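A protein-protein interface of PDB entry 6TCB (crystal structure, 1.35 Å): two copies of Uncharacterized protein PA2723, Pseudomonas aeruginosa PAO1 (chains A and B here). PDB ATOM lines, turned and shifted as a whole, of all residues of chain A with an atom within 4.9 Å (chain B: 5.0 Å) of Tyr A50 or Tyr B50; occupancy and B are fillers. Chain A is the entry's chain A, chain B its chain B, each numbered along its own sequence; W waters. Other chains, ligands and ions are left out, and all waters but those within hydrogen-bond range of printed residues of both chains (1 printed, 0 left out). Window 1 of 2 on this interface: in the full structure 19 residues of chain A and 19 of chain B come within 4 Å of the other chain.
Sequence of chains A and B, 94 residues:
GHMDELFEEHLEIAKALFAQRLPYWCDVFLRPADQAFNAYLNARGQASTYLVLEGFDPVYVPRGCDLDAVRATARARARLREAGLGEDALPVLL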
ATOM      1  N   ASP A  34      28.303 -16.545  -7.649  1.00  0.00           N
ATOM      2  CA  ASP A  34      27.870 -17.420  -6.562  1.00  0.00           C
ATOM      3  C   ASP A  34      28.925 -18.475  -6.242  1.00  0.00           C
ATOM      4  O   ASP A  34      29.282 -18.687  -5.077  1.00  0.00           O
ATOM      5  CB  ASP A  34      26.484 -18.034  -6.837  1.00  0.00           C
ATOM      6  CG  ASP A  34      26.332 -18.711  -8.203  1.00  0.00           C
ATOM      7  OD1 ASP A  34      27.272 -18.799  -9.030  1.00  0.00           O
ATOM      8  OD2 ASP A  34      25.188 -19.176  -8.463  1.00  0.00           O
ATOM      9  N   GLN A  35      29.467 -19.122  -7.270  1.00  0.00           N
ATOM     10  CA  GLN A  35      30.511 -20.117  -7.049  1.00  0.00           C
ATOM     11  C   GLN A  35      31.825 -19.454  -6.665  1.00  0.00           C
ATOM     12  O   GLN A  35      32.570 -19.970  -5.818  1.00  0.00           O
ATOM     13  CB  GLN A  35      30.701 -20.945  -8.318  1.00  0.00           C
ATOM     14  CG  GLN A  35      29.458 -21.706  -8.736  1.00  0.00           C
ATOM     15  CD  GLN A  35      29.747 -22.771  -9.774  1.00  0.00           C
ATOM     16  OE1 GLN A  35      30.418 -23.762  -9.481  1.00  0.00           O
ATOM     17  NE2 GLN A  35      29.243 -22.575 -10.989  1.00  0.00           N
ATOM     18  N   ASN A  38      32.819 -18.810  -3.044  1.00  0.00           N
ATOM     19  CA  ASN A  38      33.472 -19.853  -2.263  1.00  0.00           C
ATOM     20  C   ASN A  38      34.989 -19.778  -2.393  1.00  0.00           C
ATOM     21  O   ASN A  38      35.715 -20.009  -1.416  1.00  0.00           O
ATOM     22  CB  ASN A  38      32.957 -21.237  -2.635  1.00  0.00           C
ATOM     23  CG  ASN A  38      33.166 -22.220  -1.521  1.00  0.00           C
ATOM     24  OD1 ASN A  38      32.610 -22.059  -0.437  1.00  0.00           O
ATOM     25  ND2 ASN A  38      33.979 -23.234  -1.766  1.00  0.00           N
ATOM     26  N   SER A  48      35.729 -23.360   3.383  1.00  0.00           N
ATOM     27  CA  SER A  48      34.322 -23.443   3.032  1.00  0.00           C
ATOM     28  C   SER A  48      34.085 -24.393   1.873  1.00  0.00           C
ATOM     29  O   SER A  48      34.859 -24.429   0.912  1.00  0.00           O
ATOM     30  CB  SER A  48      33.798 -22.048   2.634  1.00  0.00           C
ATOM     31  OG  SER A  48      32.426 -22.085   2.281  1.00  0.00           O
ATOM     32  N   THR A  49      32.981 -25.128   1.976  1.00  0.00           N
ATOM     33  CA  THR A  49      32.441 -25.947   0.898  1.00  0.00           C
ATOM     34  C   THR A  49      31.157 -25.307   0.385  1.00  0.00           C
ATOM     35  O   THR A  49      30.268 -24.964   1.170  1.00  0.00           O
ATOM     36  CB  THR A  49      32.125 -27.351   1.423  1.00  0.00           C
ATOM     37  OG1 THR A  49      33.315 -27.922   1.974  1.00  0.00           O
ATOM     38  CG2 THR A  49      31.605 -28.250   0.310  1.00  0.00           C
ATOM     39  N   TYR A  50      31.042 -25.175  -0.926  1.00  0.00           N
ATOM     40  CA  TYR A  50      29.843 -24.634  -1.543  1.00  0.00           C
ATOM     41  C   TYR A  50      28.922 -25.772  -1.932  1.00  0.00           C
ATOM     42  O   TYR A  50      29.368 -26.751  -2.547  1.00  0.00           O
ATOM     43  CB  TYR A  50      30.226 -23.850  -2.784  1.00  0.00           C
ATOM     44  CG  TYR A  50      29.109 -23.283  -3.621  1.00  0.00           C
ATOM     45  CD1 TYR A  50      28.278 -22.281  -3.137  1.00  0.00           C
ATOM     46  CD2 TYR A  50      28.944 -23.699  -4.928  1.00  0.00           C
ATOM     47  CE1 TYR A  50      27.291 -21.736  -3.935  1.00  0.00           C
ATOM     48  CE2 TYR A  50      27.960 -23.158  -5.733  1.00  0.00           C
ATOM     49  CZ  TYR A  50      27.152 -22.156  -5.226  1.00  0.00           C
ATOM     50  OH  TYR A  50      26.176 -21.599  -6.027  1.00  0.00           O
ATOM     51  N   LEU A  51      27.652 -25.656  -1.562  1.00  0.00           N
ATOM     52  CA  LEU A  51      26.637 -26.604  -1.981  1.00  0.00           C
ATOM     53  C   LEU A  51      25.479 -25.845  -2.620  1.00  0.00           C
ATOM     54  O   LEU A  51      25.144 -24.728  -2.210  1.00  0.00           O
ATOM     55  CB  LEU A  51      26.044 -27.395  -0.804  1.00  0.00           C
ATOM     56  CG  LEU A  51      26.984 -28.189   0.105  1.00  0.00           C
ATOM     57  CD1 LEU A  51      26.169 -28.796   1.264  1.00  0.00           C
ATOM     58  CD2 LEU A  51      27.703 -29.251  -0.667  1.00  0.00           C
ATOM     59  N   VAL A  52      24.849 -26.453  -3.611  1.00  0.00           N
ATOM     60  CA  VAL A  52      23.530 -26.021  -4.045  1.00  0.00           C
ATOM     61  C   VAL A  52      22.589 -27.182  -3.792  1.00  0.00           C
ATOM     62  O   VAL A  52      22.805 -28.288  -4.308  1.00  0.00           O
ATOM     63  CB  VAL A  52      23.491 -25.568  -5.509  1.00  0.00           C
ATOM     64  CG1 VAL A  52      22.060 -25.156  -5.880  1.00  0.00           C
ATOM     65  CG2 VAL A  52      24.464 -24.444  -5.724  1.00  0.00           C
ATOM     66  N   PRO A  58      21.540 -22.152  -2.410  1.00  0.00           N
ATOM     67  CA  PRO A  58      22.994 -22.175  -2.230  1.00  0.00           C
ATOM     68  C   PRO A  58      23.443 -21.839  -0.818  1.00  0.00           C
ATOM     69  O   PRO A  58      22.826 -21.050  -0.099  1.00  0.00           O
ATOM     70  CB  PRO A  58      23.467 -21.078  -3.197  1.00  0.00           C
ATOM     71  CG  PRO A  58      22.320 -20.138  -3.285  1.00  0.00           C
ATOM     72  CD  PRO A  58      21.067 -20.938  -3.100  1.00  0.00           C
ATOM     73  N   VAL A  59      24.562 -22.438  -0.431  1.00  0.00           N
ATOM     74  CA  VAL A  59      25.063 -22.320   0.931  1.00  0.00           C
ATOM     75  C   VAL A  59      26.565 -22.525   0.931  1.00  0.00           C
ATOM     76  O   VAL A  59      27.106 -23.284   0.122  1.00  0.00           O
ATOM     77  CB  VAL A  59      24.312 -23.321   1.852  1.00  0.00           C
ATOM     78  CG1 VAL A  59      24.563 -24.777   1.424  1.00  0.00           C
ATOM     79  CG2 VAL A  59      24.655 -23.128   3.301  1.00  0.00           C
ATOM     80  N   TYR A  60      27.221 -21.822   1.848  1.00  0.00           N
ATOM     81  CA  TYR A  60      28.660 -21.875   2.071  1.00  0.00           C
ATOM     82  C   TYR A  60      28.849 -22.468   3.460  1.00  0.00           C
ATOM     83  O   TYR A  60      28.360 -21.903   4.442  1.00  0.00           O
ATOM     84  CB  TYR A  60      29.265 -20.467   1.948  1.00  0.00           C
ATOM     85  CG  TYR A  60      28.894 -19.831   0.626  1.00  0.00           C
ATOM     86  CD1 TYR A  60      29.664 -20.033  -0.503  1.00  0.00           C
ATOM     87  CD2 TYR A  60      27.733 -19.073   0.486  1.00  0.00           C
ATOM     88  CE1 TYR A  60      29.302 -19.493  -1.724  1.00  0.00           C
ATOM     89  CE2 TYR A  60      27.366 -18.525  -0.741  1.00  0.00           C
ATOM     90  CZ  TYR A  60      28.151 -18.754  -1.841  1.00  0.00           C
ATOM     91  OH  TYR A  60      27.742 -18.189  -3.029  1.00  0.00           O
ATOM     92  N   ASP B  34      28.301 -25.946 -15.369  1.00  0.00           N
ATOM     93  CA  ASP B  34      28.471 -26.950 -14.322  1.00  0.00           C
ATOM     94  C   ASP B  34      27.338 -26.893 -13.302  1.00  0.00           C
ATOM     95  O   ASP B  34      26.665 -27.898 -13.036  1.00  0.00           O
ATOM     96  CB  ASP B  34      29.870 -26.850 -13.668  1.00  0.00           C
ATOM     97  CG  ASP B  34      30.278 -25.429 -13.236  1.00  0.00           C
ATOM     98  OD1 ASP B  34      29.477 -24.474 -13.286  1.00  0.00           O
ATOM     99  OD2 ASP B  34      31.456 -25.261 -12.826  1.00  0.00           O
ATOM    100  N   GLN B  35      27.064 -25.711 -12.764  1.00  0.00           N
ATOM    101  CA  GLN B  35      25.989 -25.593 -11.789  1.00  0.00           C
ATOM    102  C   GLN B  35      24.630 -25.791 -12.442  1.00  0.00           C
ATOM    103  O   GLN B  35      23.732 -26.398 -11.849  1.00  0.00           O
ATOM    104  CB  GLN B  35      26.052 -24.223 -11.126  1.00  0.00           C
ATOM    105  CG  GLN B  35      25.015 -23.988 -10.060  1.00  0.00           C
ATOM    106  CD  GLN B  35      25.277 -22.702  -9.331  1.00  0.00           C
ATOM    107  OE1 GLN B  35      26.206 -22.616  -8.532  1.00  0.00           O
ATOM    108  NE2 GLN B  35      24.514 -21.678  -9.644  1.00  0.00           N
ATOM    109  N   ASN B  38      23.270 -29.300 -12.523  1.00  0.00           N
ATOM    110  CA  ASN B  38      22.610 -29.756 -11.306  1.00  0.00           C
ATOM    111  C   ASN B  38      21.156 -29.297 -11.266  1.00  0.00           C
ATOM    112  O   ASN B  38      20.263 -30.055 -10.854  1.00  0.00           O
ATOM    113  CB  ASN B  38      23.345 -29.249 -10.070  1.00  0.00           C
ATOM    114  CG  ASN B  38      22.645 -29.637  -8.806  1.00  0.00           C
ATOM    115  OD1 ASN B  38      22.652 -30.803  -8.419  1.00  0.00           O
ATOM    116  ND2 ASN B  38      22.016 -28.666  -8.152  1.00  0.00           N
ATOM    117  N   SER B  48      19.588 -34.255  -6.747  1.00  0.00           N
ATOM    118  CA  SER B  48      21.030 -34.102  -6.804  1.00  0.00           C
ATOM    119  C   SER B  48      21.424 -32.883  -5.993  1.00  0.00           C
ATOM    120  O   SER B  48      20.704 -31.884  -5.961  1.00  0.00           O
ATOM    121  CB  SER B  48      21.483 -33.895  -8.266  1.00  0.00           C
ATOM    122  OG  SER B  48      22.864 -33.635  -8.366  1.00  0.00           O
ATOM    123  N   THR B  49      22.585 -32.967  -5.362  1.00  0.00           N
ATOM    124  CA  THR B  49      23.231 -31.846  -4.697  1.00  0.00           C
ATOM    125  C   THR B  49      24.521 -31.538  -5.439  1.00  0.00           C
ATOM    126  O   THR B  49      25.293 -32.448  -5.751  1.00  0.00           O
ATOM    127  CB  THR B  49      23.572 -32.216  -3.250  1.00  0.00           C
ATOM    128  OG1 THR B  49      22.364 -32.410  -2.512  1.00  0.00           O
ATOM    129  CG2 THR B  49      24.399 -31.124  -2.579  1.00  0.00           C
ATOM    130  N   TYR B  50      24.767 -30.264  -5.710  1.00  0.00           N
ATOM    131  CA  TYR B  50      26.011 -29.817  -6.326  1.00  0.00           C
ATOM    132  C   TYR B  50      26.989 -29.424  -5.237  1.00  0.00           C
ATOM    133  O   TYR B  50      26.629 -28.711  -4.306  1.00  0.00           O
ATOM    134  CB  TYR B  50      25.700 -28.583  -7.165  1.00  0.00           C
ATOM    135  CG  TYR B  50      26.796 -27.974  -7.974  1.00  0.00           C
ATOM    136  CD1 TYR B  50      27.382 -28.659  -9.020  1.00  0.00           C
ATOM    137  CD2 TYR B  50      27.204 -26.667  -7.731  1.00  0.00           C
ATOM    138  CE1 TYR B  50      28.370 -28.068  -9.788  1.00  0.00           C
ATOM    139  CE2 TYR B  50      28.172 -26.073  -8.497  1.00  0.00           C
ATOM    140  CZ  TYR B  50      28.760 -26.782  -9.513  1.00  0.00           C
ATOM    141  OH  TYR B  50      29.732 -26.211 -10.284  1.00  0.00           O
ATOM    142  N   LEU B  51      28.236 -29.874  -5.363  1.00  0.00           N
ATOM    143  CA  LEU B  51      29.259 -29.587  -4.360  1.00  0.00           C
ATOM    144  C   LEU B  51      30.533 -29.092  -5.029  1.00  0.00           C
ATOM    145  O   LEU B  51      30.972 -29.659  -6.038  1.00  0.00           O
ATOM    146  CB  LEU B  51      29.560 -30.834  -3.513  1.00  0.00           C
ATOM    147  CG  LEU B  51      30.652 -30.731  -2.444  1.00  0.00           C
ATOM    148  CD1 LEU B  51      30.358 -31.794  -1.381  1.00  0.00           C
ATOM    149  CD2 LEU B  51      32.079 -30.911  -2.943  1.00  0.00           C
ATOM    150  N   VAL B  52      31.106 -28.025  -4.473  1.00  0.00           N
ATOM    151  CA  VAL B  52      32.359 -27.451  -4.945  1.00  0.00           C
ATOM    152  C   VAL B  52      33.254 -27.167  -3.748  1.00  0.00           C
ATOM    153  O   VAL B  52      32.839 -26.483  -2.804  1.00  0.00           O
ATOM    154  CB  VAL B  52      32.128 -26.147  -5.728  1.00  0.00           C
ATOM    155  CG1 VAL B  52      33.457 -25.598  -6.197  1.00  0.00           C
ATOM    156  CG2 VAL B  52      31.213 -26.385  -6.905  1.00  0.00           C
ATOM    157  N   PRO B  58      33.665 -30.605 -10.940  1.00  0.00           N
ATOM    158  CA  PRO B  58      32.224 -30.635 -10.663  1.00  0.00           C
ATOM    159  C   PRO B  58      31.737 -32.008 -10.237  1.00  0.00           C
ATOM    160  O   PRO B  58      32.116 -33.032 -10.810  1.00  0.00           O
ATOM    161  CB  PRO B  58      31.600 -30.212 -11.998  1.00  0.00           C
ATOM    162  CG  PRO B  58      32.646 -29.372 -12.633  1.00  0.00           C
ATOM    163  CD  PRO B  58      33.955 -30.039 -12.270  1.00  0.00           C
ATOM    164  N   VAL B  59      30.854 -32.009  -9.244  1.00  0.00           N
ATOM    165  CA  VAL B  59      30.279 -33.237  -8.721  1.00  0.00           C
ATOM    166  C   VAL B  59      28.808 -33.029  -8.390  1.00  0.00           C
ATOM    167  O   VAL B  59      28.389 -31.975  -7.902  1.00  0.00           O
ATOM    168  CB  VAL B  59      31.099 -33.782  -7.530  1.00  0.00           C
ATOM    169  CG1 VAL B  59      30.876 -32.952  -6.281  1.00  0.00           C
ATOM    170  CG2 VAL B  59      30.784 -35.254  -7.290  1.00  0.00           C
ATOM    171  N   TYR B  60      28.038 -34.069  -8.675  1.00  0.00           N
ATOM    172  CA  TYR B  60      26.583 -34.140  -8.531  1.00  0.00           C
ATOM    173  C   TYR B  60      26.305 -35.364  -7.673  1.00  0.00           C
ATOM    174  O   TYR B  60      26.685 -36.479  -8.044  1.00  0.00           O
ATOM    175  CB  TYR B  60      25.933 -34.279  -9.924  1.00  0.00           C
ATOM    176  CG  TYR B  60      26.443 -33.198 -10.847  1.00  0.00           C
ATOM    177  CD1 TYR B  60      25.920 -31.914 -10.815  1.00  0.00           C
ATOM    178  CD2 TYR B  60      27.525 -33.425 -11.668  1.00  0.00           C
ATOM    179  CE1 TYR B  60      26.450 -30.897 -11.612  1.00  0.00           C
ATOM    180  CE2 TYR B  60      28.046 -32.435 -12.471  1.00  0.00           C
ATOM    181  CZ  TYR B  60      27.515 -31.169 -12.436  1.00  0.00           C
ATOM    182  OH  TYR B  60      28.051 -30.178 -13.230  1.00  0.00           O
HETATM  183  O   HOH W   1      20.622 -29.231  -5.649  1.00  0.00           O
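OD2 of Asp A34 sits at hydrogen-bond distance from NE2 of Gln B35 (2.8 Å). NE2 of Gln A35 sits at hydrogen-bond distance from OD1 of Asp B34 (3.0 Å). OE1 of Gln A35 sits at hydrogen-bond distance from OH of Tyr B50 (2.7 Å). The side-chain hydroxyl (OH) of Tyr A50 is in hydrogen-bond range of the side-chain amide oxygen (OE1) of Gln B35, 2.7 Å away. The backbone NH (N) of Val B52 is in hydrogen-bond range of the backbone carbonyl oxygen (O) of Tyr A50, 2.9 Å away. N of Val A52 lies within hydrogen-bond range of O of Tyr B50, 3.0 Å away.
OH of Tyr A60 sits at hydrogen-bond distance from O of Asp A34. O of Leu A51 lies within hydrogen-bond range of N of Val A59 (3.0 Å). The side-chain carboxylate of Asp B34 sits close to the side-chain hydroxyl of Tyr B50 (3.2 Å). The backbone carbonyl oxygen (O) of Asp B34 is in hydrogen-bond range of the side-chain hydroxyl (OH) of Tyr B60 (2.7 Å). The side-chain amide oxygen (OD1) of Asn B38 is in hydrogen-bond range of the side-chain hydroxyl (OG) of Ser B48, 2.8 Å away. The backbone NH of Leu B51 lies within hydrogen-bond range of the backbone carbonyl oxygen of Val B59 (3.3 Å).
CG of Gln A35 touches OE1 of Gln B35, 3.4 Å away. Gln A35 touches Val B52 (OE1 to CG2, 3.8 Å). Thr A49 touches Leu B51. Val B52 touches Thr A49. O of Tyr A50 touches O of Tyr B50, 3.8 Å away. Tyr A50 touches Leu B51 (O to CA, 3.4 Å). O of Tyr B50 touches CA of Leu A51 (3.1 Å). Leu A51 touches Leu B51 (CD2 to CD1, 3.7 Å). Gln B35 touches Val A52 (OE1 to CG2, 3.8 Å). Val A52 touches Asn B38 (O to ND2, 3.9 Å).
Printed residues of chain B within 4 Å of Gln A35: Asp B34 (3.0 Å), Gln B35 (3.4 Å), Tyr B50 (2.7 Å) and Val B52 (3.8 Å). Tyr A50 touches just these residues of chain B: Gln B35 (2.7 Å), Tyr B50 (3.8 Å), Leu B51 (3.4 Å) and Val B52 (2.9 Å). Printed residues of chain A within 4 Å of Asn B38: Val A52 (3.9 Å). Of the printed residues of chain A, Thr B49 touches Val A52 (3.6 Å). Pro B58 touches none of the printed residues of chain A.
Of the 11 printed residues of chain B, 7 touch a printed residue of chain A. Printed residues of chain B that touch a printed residue of chain A: Asp B34, Gln B35, Asn B38, Thr B49, Tyr B50, Leu B51 and Val B52. Hydrophobic or aromatic side chains of chain B within 4 Å of the printed part of chain A: Tyr B50, Leu B51 and Val B52. Printed residues of chain A that touch a printed residue of chain B: Asp A34, Gln A35, Asn A38, Thr A49, Tyr A50, Leu A51 and Val A52. Hydrophobic or aromatic side chains of chain A within 4 Å of the printed part of chain B: Tyr A50, Leu A51 and Val A52. Among the printed residues, no Asp or Glu carboxylate lies within 4 Å of a Lys or Arg side-chain nitrogen of the other chain.
Gln A35 touches Tyr B50, and with the chains exchanged Tyr A50 touches Gln B35. Asn A38 touches Val B52, and with the chains exchanged Val A52 touches Asn B38. Thr A49 touches Val B52, and with the chains exchanged Val A52 touches Thr B49. Leu B51 touches its own counterpart, Leu A51.
Water W1 lies within hydrogen-bond range of O of Ser B48, O of Val A52 and ND2 of Asn B38.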
